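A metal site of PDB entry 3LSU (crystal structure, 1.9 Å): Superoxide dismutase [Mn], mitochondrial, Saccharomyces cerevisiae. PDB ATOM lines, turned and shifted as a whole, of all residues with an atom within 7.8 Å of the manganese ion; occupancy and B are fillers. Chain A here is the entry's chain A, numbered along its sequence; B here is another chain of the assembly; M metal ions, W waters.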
ATOM      1  N   HIS A  26     -21.369  26.746 -34.748  1.00  0.00           N
ATOM      2  CA  HIS A  26     -22.550  26.553 -33.910  1.00  0.00           C
ATOM      3  C   HIS A  26     -23.601  25.683 -34.623  1.00  0.00           C
ATOM      4  O   HIS A  26     -24.159  24.752 -34.025  1.00  0.00           O
ATOM      5  CB  HIS A  26     -23.137  27.902 -33.531  1.00  0.00           C
ATOM      6  CG  HIS A  26     -23.929  27.874 -32.263  1.00  0.00           C
ATOM      7  ND1 HIS A  26     -24.566  28.993 -31.760  1.00  0.00           N
ATOM      8  CD2 HIS A  26     -24.172  26.875 -31.388  1.00  0.00           C
ATOM      9  CE1 HIS A  26     -25.172  28.665 -30.631  1.00  0.00           C
ATOM     10  NE2 HIS A  26     -24.960  27.391 -30.395  1.00  0.00           N
ATOM     11  N   TYR A  27     -23.836  25.970 -35.895  1.00  0.00           N
ATOM     12  CA  TYR A  27     -24.831  25.262 -36.705  1.00  0.00           C
ATOM     13  C   TYR A  27     -24.308  23.932 -37.275  1.00  0.00           C
ATOM     14  O   TYR A  27     -24.932  22.876 -37.094  1.00  0.00           O
ATOM     15  CB  TYR A  27     -25.293  26.193 -37.837  1.00  0.00           C
ATOM     16  CG  TYR A  27     -26.326  25.660 -38.819  1.00  0.00           C
ATOM     17  CD1 TYR A  27     -27.687  25.707 -38.517  1.00  0.00           C
ATOM     18  CD2 TYR A  27     -25.942  25.171 -40.067  1.00  0.00           C
ATOM     19  CE1 TYR A  27     -28.636  25.248 -39.427  1.00  0.00           C
ATOM     20  CE2 TYR A  27     -26.891  24.722 -40.994  1.00  0.00           C
ATOM     21  CZ  TYR A  27     -28.233  24.762 -40.661  1.00  0.00           C
ATOM     22  OH  TYR A  27     -29.184  24.314 -41.563  1.00  0.00           O
ATOM     23  N   HIS A  30     -22.142  21.954 -33.619  1.00  0.00           N
ATOM     24  CA  HIS A  30     -22.910  21.776 -32.378  1.00  0.00           C
ATOM     25  C   HIS A  30     -24.355  21.342 -32.597  1.00  0.00           C
ATOM     26  O   HIS A  30     -24.793  20.340 -32.023  1.00  0.00           O
ATOM     27  CB  HIS A  30     -22.832  23.022 -31.495  1.00  0.00           C
ATOM     28  CG  HIS A  30     -21.451  23.356 -31.042  1.00  0.00           C
ATOM     29  ND1 HIS A  30     -20.844  22.718 -29.981  1.00  0.00           N
ATOM     30  CD2 HIS A  30     -20.531  24.232 -31.511  1.00  0.00           C
ATOM     31  CE1 HIS A  30     -19.632  23.199 -29.802  1.00  0.00           C
ATOM     32  NE2 HIS A  30     -19.410  24.128 -30.722  1.00  0.00           N
ATOM     33  N   HIS A  31     -25.115  22.086 -33.396  1.00  0.00           N
ATOM     34  CA  HIS A  31     -26.502  21.718 -33.656  1.00  0.00           C
ATOM     35  C   HIS A  31     -26.587  20.371 -34.377  1.00  0.00           C
ATOM     36  O   HIS A  31     -27.470  19.552 -34.087  1.00  0.00           O
ATOM     37  CB  HIS A  31     -27.238  22.803 -34.470  1.00  0.00           C
ATOM     38  CG  HIS A  31     -28.737  22.711 -34.403  1.00  0.00           C
ATOM     39  ND1 HIS A  31     -29.562  23.603 -35.031  1.00  0.00           N
ATOM     40  CD2 HIS A  31     -29.548  21.821 -33.763  1.00  0.00           C
ATOM     41  CE1 HIS A  31     -30.829  23.288 -34.789  1.00  0.00           C
ATOM     42  NE2 HIS A  31     -30.843  22.207 -34.017  1.00  0.00           N
ATOM     43  N   TYR A  34     -26.443  17.503 -31.935  1.00  0.00           N
ATOM     44  CA  TYR A  34     -27.704  17.217 -31.254  1.00  0.00           C
ATOM     45  C   TYR A  34     -28.689  16.534 -32.203  1.00  0.00           C
ATOM     46  O   TYR A  34     -29.482  15.698 -31.781  1.00  0.00           O
ATOM     47  CB  TYR A  34     -28.326  18.476 -30.671  1.00  0.00           C
ATOM     48  CG  TYR A  34     -27.411  19.184 -29.692  1.00  0.00           C
ATOM     49  CD1 TYR A  34     -26.919  18.502 -28.575  1.00  0.00           C
ATOM     50  CD2 TYR A  34     -27.050  20.512 -29.859  1.00  0.00           C
ATOM     51  CE1 TYR A  34     -26.082  19.145 -27.664  1.00  0.00           C
ATOM     52  CE2 TYR A  34     -26.211  21.149 -28.964  1.00  0.00           C
ATOM     53  CZ  TYR A  34     -25.730  20.459 -27.864  1.00  0.00           C
ATOM     54  OH  TYR A  34     -24.905  21.087 -26.962  1.00  0.00           O
ATOM     55  N   GLY A  77     -31.238  19.892 -27.119  1.00  0.00           N
ATOM     56  CA  GLY A  77     -30.261  20.563 -27.975  1.00  0.00           C
ATOM     57  C   GLY A  77     -30.809  20.854 -29.362  1.00  0.00           C
ATOM     58  O   GLY A  77     -30.577  21.944 -29.938  1.00  0.00           O
ATOM     59  N   ASN A  80     -33.886  23.495 -28.739  1.00  0.00           N
ATOM     60  CA  ASN A  80     -33.404  24.805 -28.296  1.00  0.00           C
ATOM     61  C   ASN A  80     -32.729  25.599 -29.417  1.00  0.00           C
ATOM     62  O   ASN A  80     -32.953  26.798 -29.570  1.00  0.00           O
ATOM     63  CB  ASN A  80     -32.484  24.672 -27.070  1.00  0.00           C
ATOM     64  CG  ASN A  80     -33.236  24.405 -25.780  1.00  0.00           C
ATOM     65  OD1 ASN A  80     -34.424  24.750 -25.642  1.00  0.00           O
ATOM     66  ND2 ASN A  80     -32.559  23.784 -24.816  1.00  0.00           N
ATOM     67  N   HIS A  81     -31.888  24.935 -30.208  1.00  0.00           N
ATOM     68  CA  HIS A  81     -31.197  25.644 -31.289  1.00  0.00           C
ATOM     69  C   HIS A  81     -32.147  26.028 -32.433  1.00  0.00           C
ATOM     70  O   HIS A  81     -31.999  27.106 -33.016  1.00  0.00           O
ATOM     71  CB  HIS A  81     -29.961  24.879 -31.765  1.00  0.00           C
ATOM     72  CG  HIS A  81     -28.868  24.820 -30.743  1.00  0.00           C
ATOM     73  ND1 HIS A  81     -28.847  23.887 -29.729  1.00  0.00           N
ATOM     74  CD2 HIS A  81     -27.798  25.621 -30.531  1.00  0.00           C
ATOM     75  CE1 HIS A  81     -27.789  24.088 -28.967  1.00  0.00           C
ATOM     76  NE2 HIS A  81     -27.140  25.143 -29.424  1.00  0.00           N
ATOM     77  N   PHE A  84     -33.650  29.140 -31.231  1.00  0.00           N
ATOM     78  CA  PHE A  84     -32.618  30.190 -31.238  1.00  0.00           C
ATOM     79  C   PHE A  84     -32.479  30.798 -32.635  1.00  0.00           C
ATOM     80  O   PHE A  84     -32.625  32.014 -32.802  1.00  0.00           O
ATOM     81  CB  PHE A  84     -31.301  29.565 -30.759  1.00  0.00           C
ATOM     82  CG  PHE A  84     -30.204  30.540 -30.492  1.00  0.00           C
ATOM     83  CD1 PHE A  84     -30.402  31.636 -29.648  1.00  0.00           C
ATOM     84  CD2 PHE A  84     -28.928  30.338 -31.028  1.00  0.00           C
ATOM     85  CE1 PHE A  84     -29.356  32.522 -29.379  1.00  0.00           C
ATOM     86  CE2 PHE A  84     -27.891  31.224 -30.748  1.00  0.00           C
ATOM     87  CZ  PHE A  84     -28.100  32.311 -29.921  1.00  0.00           C
ATOM     88  N   TRP A  85     -32.220  29.985 -33.653  1.00  0.00           N
ATOM     89  CA  TRP A  85     -32.021  30.534 -34.993  1.00  0.00           C
ATOM     90  C   TRP A  85     -33.236  31.343 -35.459  1.00  0.00           C
ATOM     91  O   TRP A  85     -33.088  32.372 -36.123  1.00  0.00           O
ATOM     92  CB  TRP A  85     -31.721  29.452 -36.034  1.00  0.00           C
ATOM     93  CG  TRP A  85     -30.651  28.478 -35.688  1.00  0.00           C
ATOM     94  CD1 TRP A  85     -30.724  27.116 -35.797  1.00  0.00           C
ATOM     95  CD2 TRP A  85     -29.341  28.770 -35.167  1.00  0.00           C
ATOM     96  NE1 TRP A  85     -29.538  26.545 -35.388  1.00  0.00           N
ATOM     97  CE2 TRP A  85     -28.676  27.534 -34.992  1.00  0.00           C
ATOM     98  CE3 TRP A  85     -28.665  29.950 -34.845  1.00  0.00           C
ATOM     99  CZ2 TRP A  85     -27.367  27.445 -34.494  1.00  0.00           C
ATOM    100  CZ3 TRP A  85     -27.364  29.861 -34.336  1.00  0.00           C
ATOM    101  CH2 TRP A  85     -26.733  28.620 -34.176  1.00  0.00           C
ATOM    102  N   GLY A 132     -26.145  26.717 -20.215  1.00  0.00           N
ATOM    103  CA  GLY A 132     -27.592  26.819 -20.152  1.00  0.00           C
ATOM    104  C   GLY A 132     -28.190  27.855 -21.070  1.00  0.00           C
ATOM    105  O   GLY A 132     -27.527  28.316 -22.004  1.00  0.00           O
ATOM    106  N   TRP A 133     -29.433  28.234 -20.778  1.00  0.00           N
ATOM    107  CA  TRP A 133     -30.246  29.115 -21.606  1.00  0.00           C
ATOM    108  C   TRP A 133     -31.020  30.044 -20.700  1.00  0.00           C
ATOM    109  O   TRP A 133     -31.274  29.726 -19.531  1.00  0.00           O
ATOM    110  CB  TRP A 133     -31.265  28.276 -22.406  1.00  0.00           C
ATOM    111  CG  TRP A 133     -30.638  27.398 -23.421  1.00  0.00           C
ATOM    112  CD1 TRP A 133     -30.056  26.169 -23.217  1.00  0.00           C
ATOM    113  CD2 TRP A 133     -30.515  27.671 -24.823  1.00  0.00           C
ATOM    114  NE1 TRP A 133     -29.577  25.673 -24.399  1.00  0.00           N
ATOM    115  CE2 TRP A 133     -29.846  26.571 -25.398  1.00  0.00           C
ATOM    116  CE3 TRP A 133     -30.902  28.724 -25.636  1.00  0.00           C
ATOM    117  CZ2 TRP A 133     -29.555  26.502 -26.763  1.00  0.00           C
ATOM    118  CZ3 TRP A 133     -30.608  28.668 -26.981  1.00  0.00           C
ATOM    119  CH2 TRP A 133     -29.947  27.561 -27.536  1.00  0.00           C
ATOM    120  N   ASN A 153     -27.880  23.326 -19.174  1.00  0.00           N
ATOM    121  CA  ASN A 153     -27.530  22.306 -20.150  1.00  0.00           C
ATOM    122  C   ASN A 153     -28.445  22.405 -21.374  1.00  0.00           C
ATOM    123  O   ASN A 153     -28.563  23.487 -21.953  1.00  0.00           O
ATOM    124  CB  ASN A 153     -27.539  20.923 -19.505  1.00  0.00           C
ATOM    125  CG  ASN A 153     -26.612  20.860 -18.306  1.00  0.00           C
ATOM    126  OD1 ASN A 153     -26.937  20.276 -17.263  1.00  0.00           O
ATOM    127  ND2 ASN A 153     -25.462  21.513 -18.419  1.00  0.00           N
ATOM    128  N   GLN A 154     -29.093  21.319 -21.765  1.00  0.00           N
ATOM    129  CA  GLN A 154     -30.069  21.414 -22.859  1.00  0.00           C
ATOM    130  C   GLN A 154     -31.502  21.196 -22.373  1.00  0.00           C
ATOM    131  O   GLN A 154     -32.388  20.819 -23.156  1.00  0.00           O
ATOM    132  CB  GLN A 154     -29.708  20.481 -24.029  1.00  0.00           C
ATOM    133  CG  GLN A 154     -28.410  20.863 -24.790  1.00  0.00           C
ATOM    134  CD  GLN A 154     -28.441  22.278 -25.365  1.00  0.00           C
ATOM    135  OE1 GLN A 154     -29.495  22.906 -25.496  1.00  0.00           O
ATOM    136  NE2 GLN A 154     -27.265  22.798 -25.711  1.00  0.00           N
ATOM    137  N   ASP A 168     -28.953  31.563 -26.024  1.00  0.00           N
ATOM    138  CA  ASP A 168     -27.969  30.542 -25.673  1.00  0.00           C
ATOM    139  C   ASP A 168     -26.860  31.099 -24.783  1.00  0.00           C
ATOM    140  O   ASP A 168     -26.214  32.069 -25.153  1.00  0.00           O
ATOM    141  CB  ASP A 168     -27.369  29.971 -26.964  1.00  0.00           C
ATOM    142  CG  ASP A 168     -26.613  28.673 -26.747  1.00  0.00           C
ATOM    143  OD1 ASP A 168     -26.475  28.229 -25.579  1.00  0.00           O
ATOM    144  OD2 ASP A 168     -26.180  28.089 -27.758  1.00  0.00           O
ATOM    145  N   ALA A 169     -26.624  30.476 -23.626  1.00  0.00           N
ATOM    146  CA  ALA A 169     -25.564  30.928 -22.734  1.00  0.00           C
ATOM    147  C   ALA A 169     -24.426  29.920 -22.603  1.00  0.00           C
ATOM    148  O   ALA A 169     -23.551  30.087 -21.754  1.00  0.00           O
ATOM    149  CB  ALA A 169     -26.136  31.285 -21.332  1.00  0.00           C
ATOM    150  N   TRP A 170     -24.446  28.866 -23.407  1.00  0.00           N
ATOM    151  CA  TRP A 170     -23.290  27.958 -23.473  1.00  0.00           C
ATOM    152  C   TRP A 170     -22.082  28.745 -23.978  1.00  0.00           C
ATOM    153  O   TRP A 170     -22.217  29.591 -24.869  1.00  0.00           O
ATOM    154  CB  TRP A 170     -23.540  26.824 -24.461  1.00  0.00           C
ATOM    155  CG  TRP A 170     -24.378  25.698 -23.942  1.00  0.00           C
ATOM    156  CD1 TRP A 170     -25.669  25.761 -23.486  1.00  0.00           C
ATOM    157  CD2 TRP A 170     -23.993  24.326 -23.868  1.00  0.00           C
ATOM    158  NE1 TRP A 170     -26.097  24.514 -23.109  1.00  0.00           N
ATOM    159  CE2 TRP A 170     -25.078  23.610 -23.340  1.00  0.00           C
ATOM    160  CE3 TRP A 170     -22.811  23.629 -24.179  1.00  0.00           C
ATOM    161  CZ2 TRP A 170     -25.034  22.224 -23.118  1.00  0.00           C
ATOM    162  CZ3 TRP A 170     -22.775  22.254 -23.961  1.00  0.00           C
ATOM    163  CH2 TRP A 170     -23.879  21.570 -23.436  1.00  0.00           C
ATOM    164  N   GLU A 171     -20.902  28.436 -23.446  1.00  0.00           N
ATOM    165  CA  GLU A 171     -19.709  29.177 -23.861  1.00  0.00           C
ATOM    166  C   GLU A 171     -19.432  29.084 -25.351  1.00  0.00           C
ATOM    167  O   GLU A 171     -18.893  30.025 -25.918  1.00  0.00           O
ATOM    168  CB  GLU A 171     -18.481  28.751 -23.035  1.00  0.00           C
ATOM    169  CG  GLU A 171     -18.613  29.150 -21.572  1.00  0.00           C
ATOM    170  CD  GLU A 171     -17.455  28.651 -20.721  1.00  0.00           C
ATOM    171  OE1 GLU A 171     -17.087  27.461 -20.838  1.00  0.00           O
ATOM    172  OE2 GLU A 171     -16.911  29.446 -19.911  1.00  0.00           O
ATOM    173  N   HIS A 172     -19.810  27.985 -26.003  1.00  0.00           N
ATOM    174  CA  HIS A 172     -19.566  27.883 -27.438  1.00  0.00           C
ATOM    175  C   HIS A 172     -20.347  28.933 -28.250  1.00  0.00           C
ATOM    176  O   HIS A 172     -20.003  29.200 -29.394  1.00  0.00           O
ATOM    177  CB  HIS A 172     -19.799  26.453 -27.974  1.00  0.00           C
ATOM    178  CG  HIS A 172     -21.231  26.019 -27.941  1.00  0.00           C
ATOM    179  ND1 HIS A 172     -21.648  24.896 -27.255  1.00  0.00           N
ATOM    180  CD2 HIS A 172     -22.343  26.560 -28.489  1.00  0.00           C
ATOM    181  CE1 HIS A 172     -22.951  24.766 -27.382  1.00  0.00           C
ATOM    182  NE2 HIS A 172     -23.402  25.765 -28.122  1.00  0.00           N
ATOM    183  N   ALA A 173     -21.365  29.547 -27.647  1.00  0.00           N
ATOM    184  CA  ALA A 173     -22.147  30.572 -28.332  1.00  0.00           C
ATOM    185  C   ALA A 173     -21.432  31.922 -28.475  1.00  0.00           C
ATOM    186  O   ALA A 173     -21.857  32.772 -29.266  1.00  0.00           O
ATOM    187  CB  ALA A 173     -23.488  30.778 -27.626  1.00  0.00           C
ATOM    188  N   TYR A 185     -21.336  39.759 -24.652  1.00  0.00           N
ATOM    189  CA  TYR A 185     -22.165  38.966 -25.567  1.00  0.00           C
ATOM    190  C   TYR A 185     -23.659  39.123 -25.240  1.00  0.00           C
ATOM    191  O   TYR A 185     -24.467  39.372 -26.138  1.00  0.00           O
ATOM    192  CB  TYR A 185     -21.743  37.487 -25.492  1.00  0.00           C
ATOM    193  CG  TYR A 185     -22.766  36.506 -26.026  1.00  0.00           C
ATOM    194  CD1 TYR A 185     -23.066  36.448 -27.382  1.00  0.00           C
ATOM    195  CD2 TYR A 185     -23.404  35.620 -25.170  1.00  0.00           C
ATOM    196  CE1 TYR A 185     -23.994  35.534 -27.873  1.00  0.00           C
ATOM    197  CE2 TYR A 185     -24.340  34.706 -25.649  1.00  0.00           C
ATOM    198  CZ  TYR A 185     -24.629  34.667 -27.004  1.00  0.00           C
ATOM    199  OH  TYR A 185     -25.560  33.748 -27.463  1.00  0.00           O
ATOM    200  N   GLU B 171     -16.150  24.252 -21.717  1.00  0.00           N
ATOM    201  CA  GLU B 171     -15.698  24.674 -23.035  1.00  0.00           C
ATOM    202  C   GLU B 171     -14.584  25.714 -22.976  1.00  0.00           C
ATOM    203  O   GLU B 171     -13.674  25.699 -23.818  1.00  0.00           O
ATOM    204  CB  GLU B 171     -16.884  25.139 -23.908  1.00  0.00           C
ATOM    205  CG  GLU B 171     -17.925  24.028 -24.109  1.00  0.00           C
ATOM    206  CD  GLU B 171     -19.129  24.456 -24.970  1.00  0.00           C
ATOM    207  OE1 GLU B 171     -19.794  25.455 -24.606  1.00  0.00           O
ATOM    208  OE2 GLU B 171     -19.413  23.777 -25.981  1.00  0.00           O
HETATM  209 MN    MN M   1     -25.526  26.298 -28.490  1.00  0.00          MN
HETATM  210  O   HOH W   1     -26.172  25.441 -26.392  1.00  0.00           O
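The side-chain carboxylate (OD1) of Asp 168 lies within hydrogen-bond range of the backbone NH (N) of Trp 170 (3.0 Å).
The backbone carbonyl oxygen of Asp 168 is in hydrogen-bond range of the side-chain hydroxyl of Tyr 185 (2.9 Å).
The indole nitrogen of Trp 85 sits close to the backbone carbonyl oxygen of His 81, at 3.5 Å.
ND1 of His 81 sits at hydrogen-bond distance from O of Gly 77.
ND1 of His 172 lies within hydrogen-bond range of OE2 of Glu 171 of chain B (2.8 Å).
O of His 26 lies within hydrogen-bond range of N of His 31 (2.9 Å).
Within 4 Å of the manganese ion: His 26, His 81, Asp 168 and His 172.
The manganese ion is bound by OD2 of Asp 168 (2.0 Å).
The manganese ion is bound by a ring nitrogen (NE2) of His 81, at 2.2 Å.
The manganese ion is bound by a ring nitrogen (NE2) of His 172, at 2.2 Å.
NE2 of His 26 binds the manganese ion (2.3 Å).
The manganese ion is bound by water W1.
Water W1 lies within hydrogen-bond range of OD1 of Asp 168 (2.9 Å), NE2 of Gln 154 (2.9 Å) and NE1 of Trp 170 (3.4 Å).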
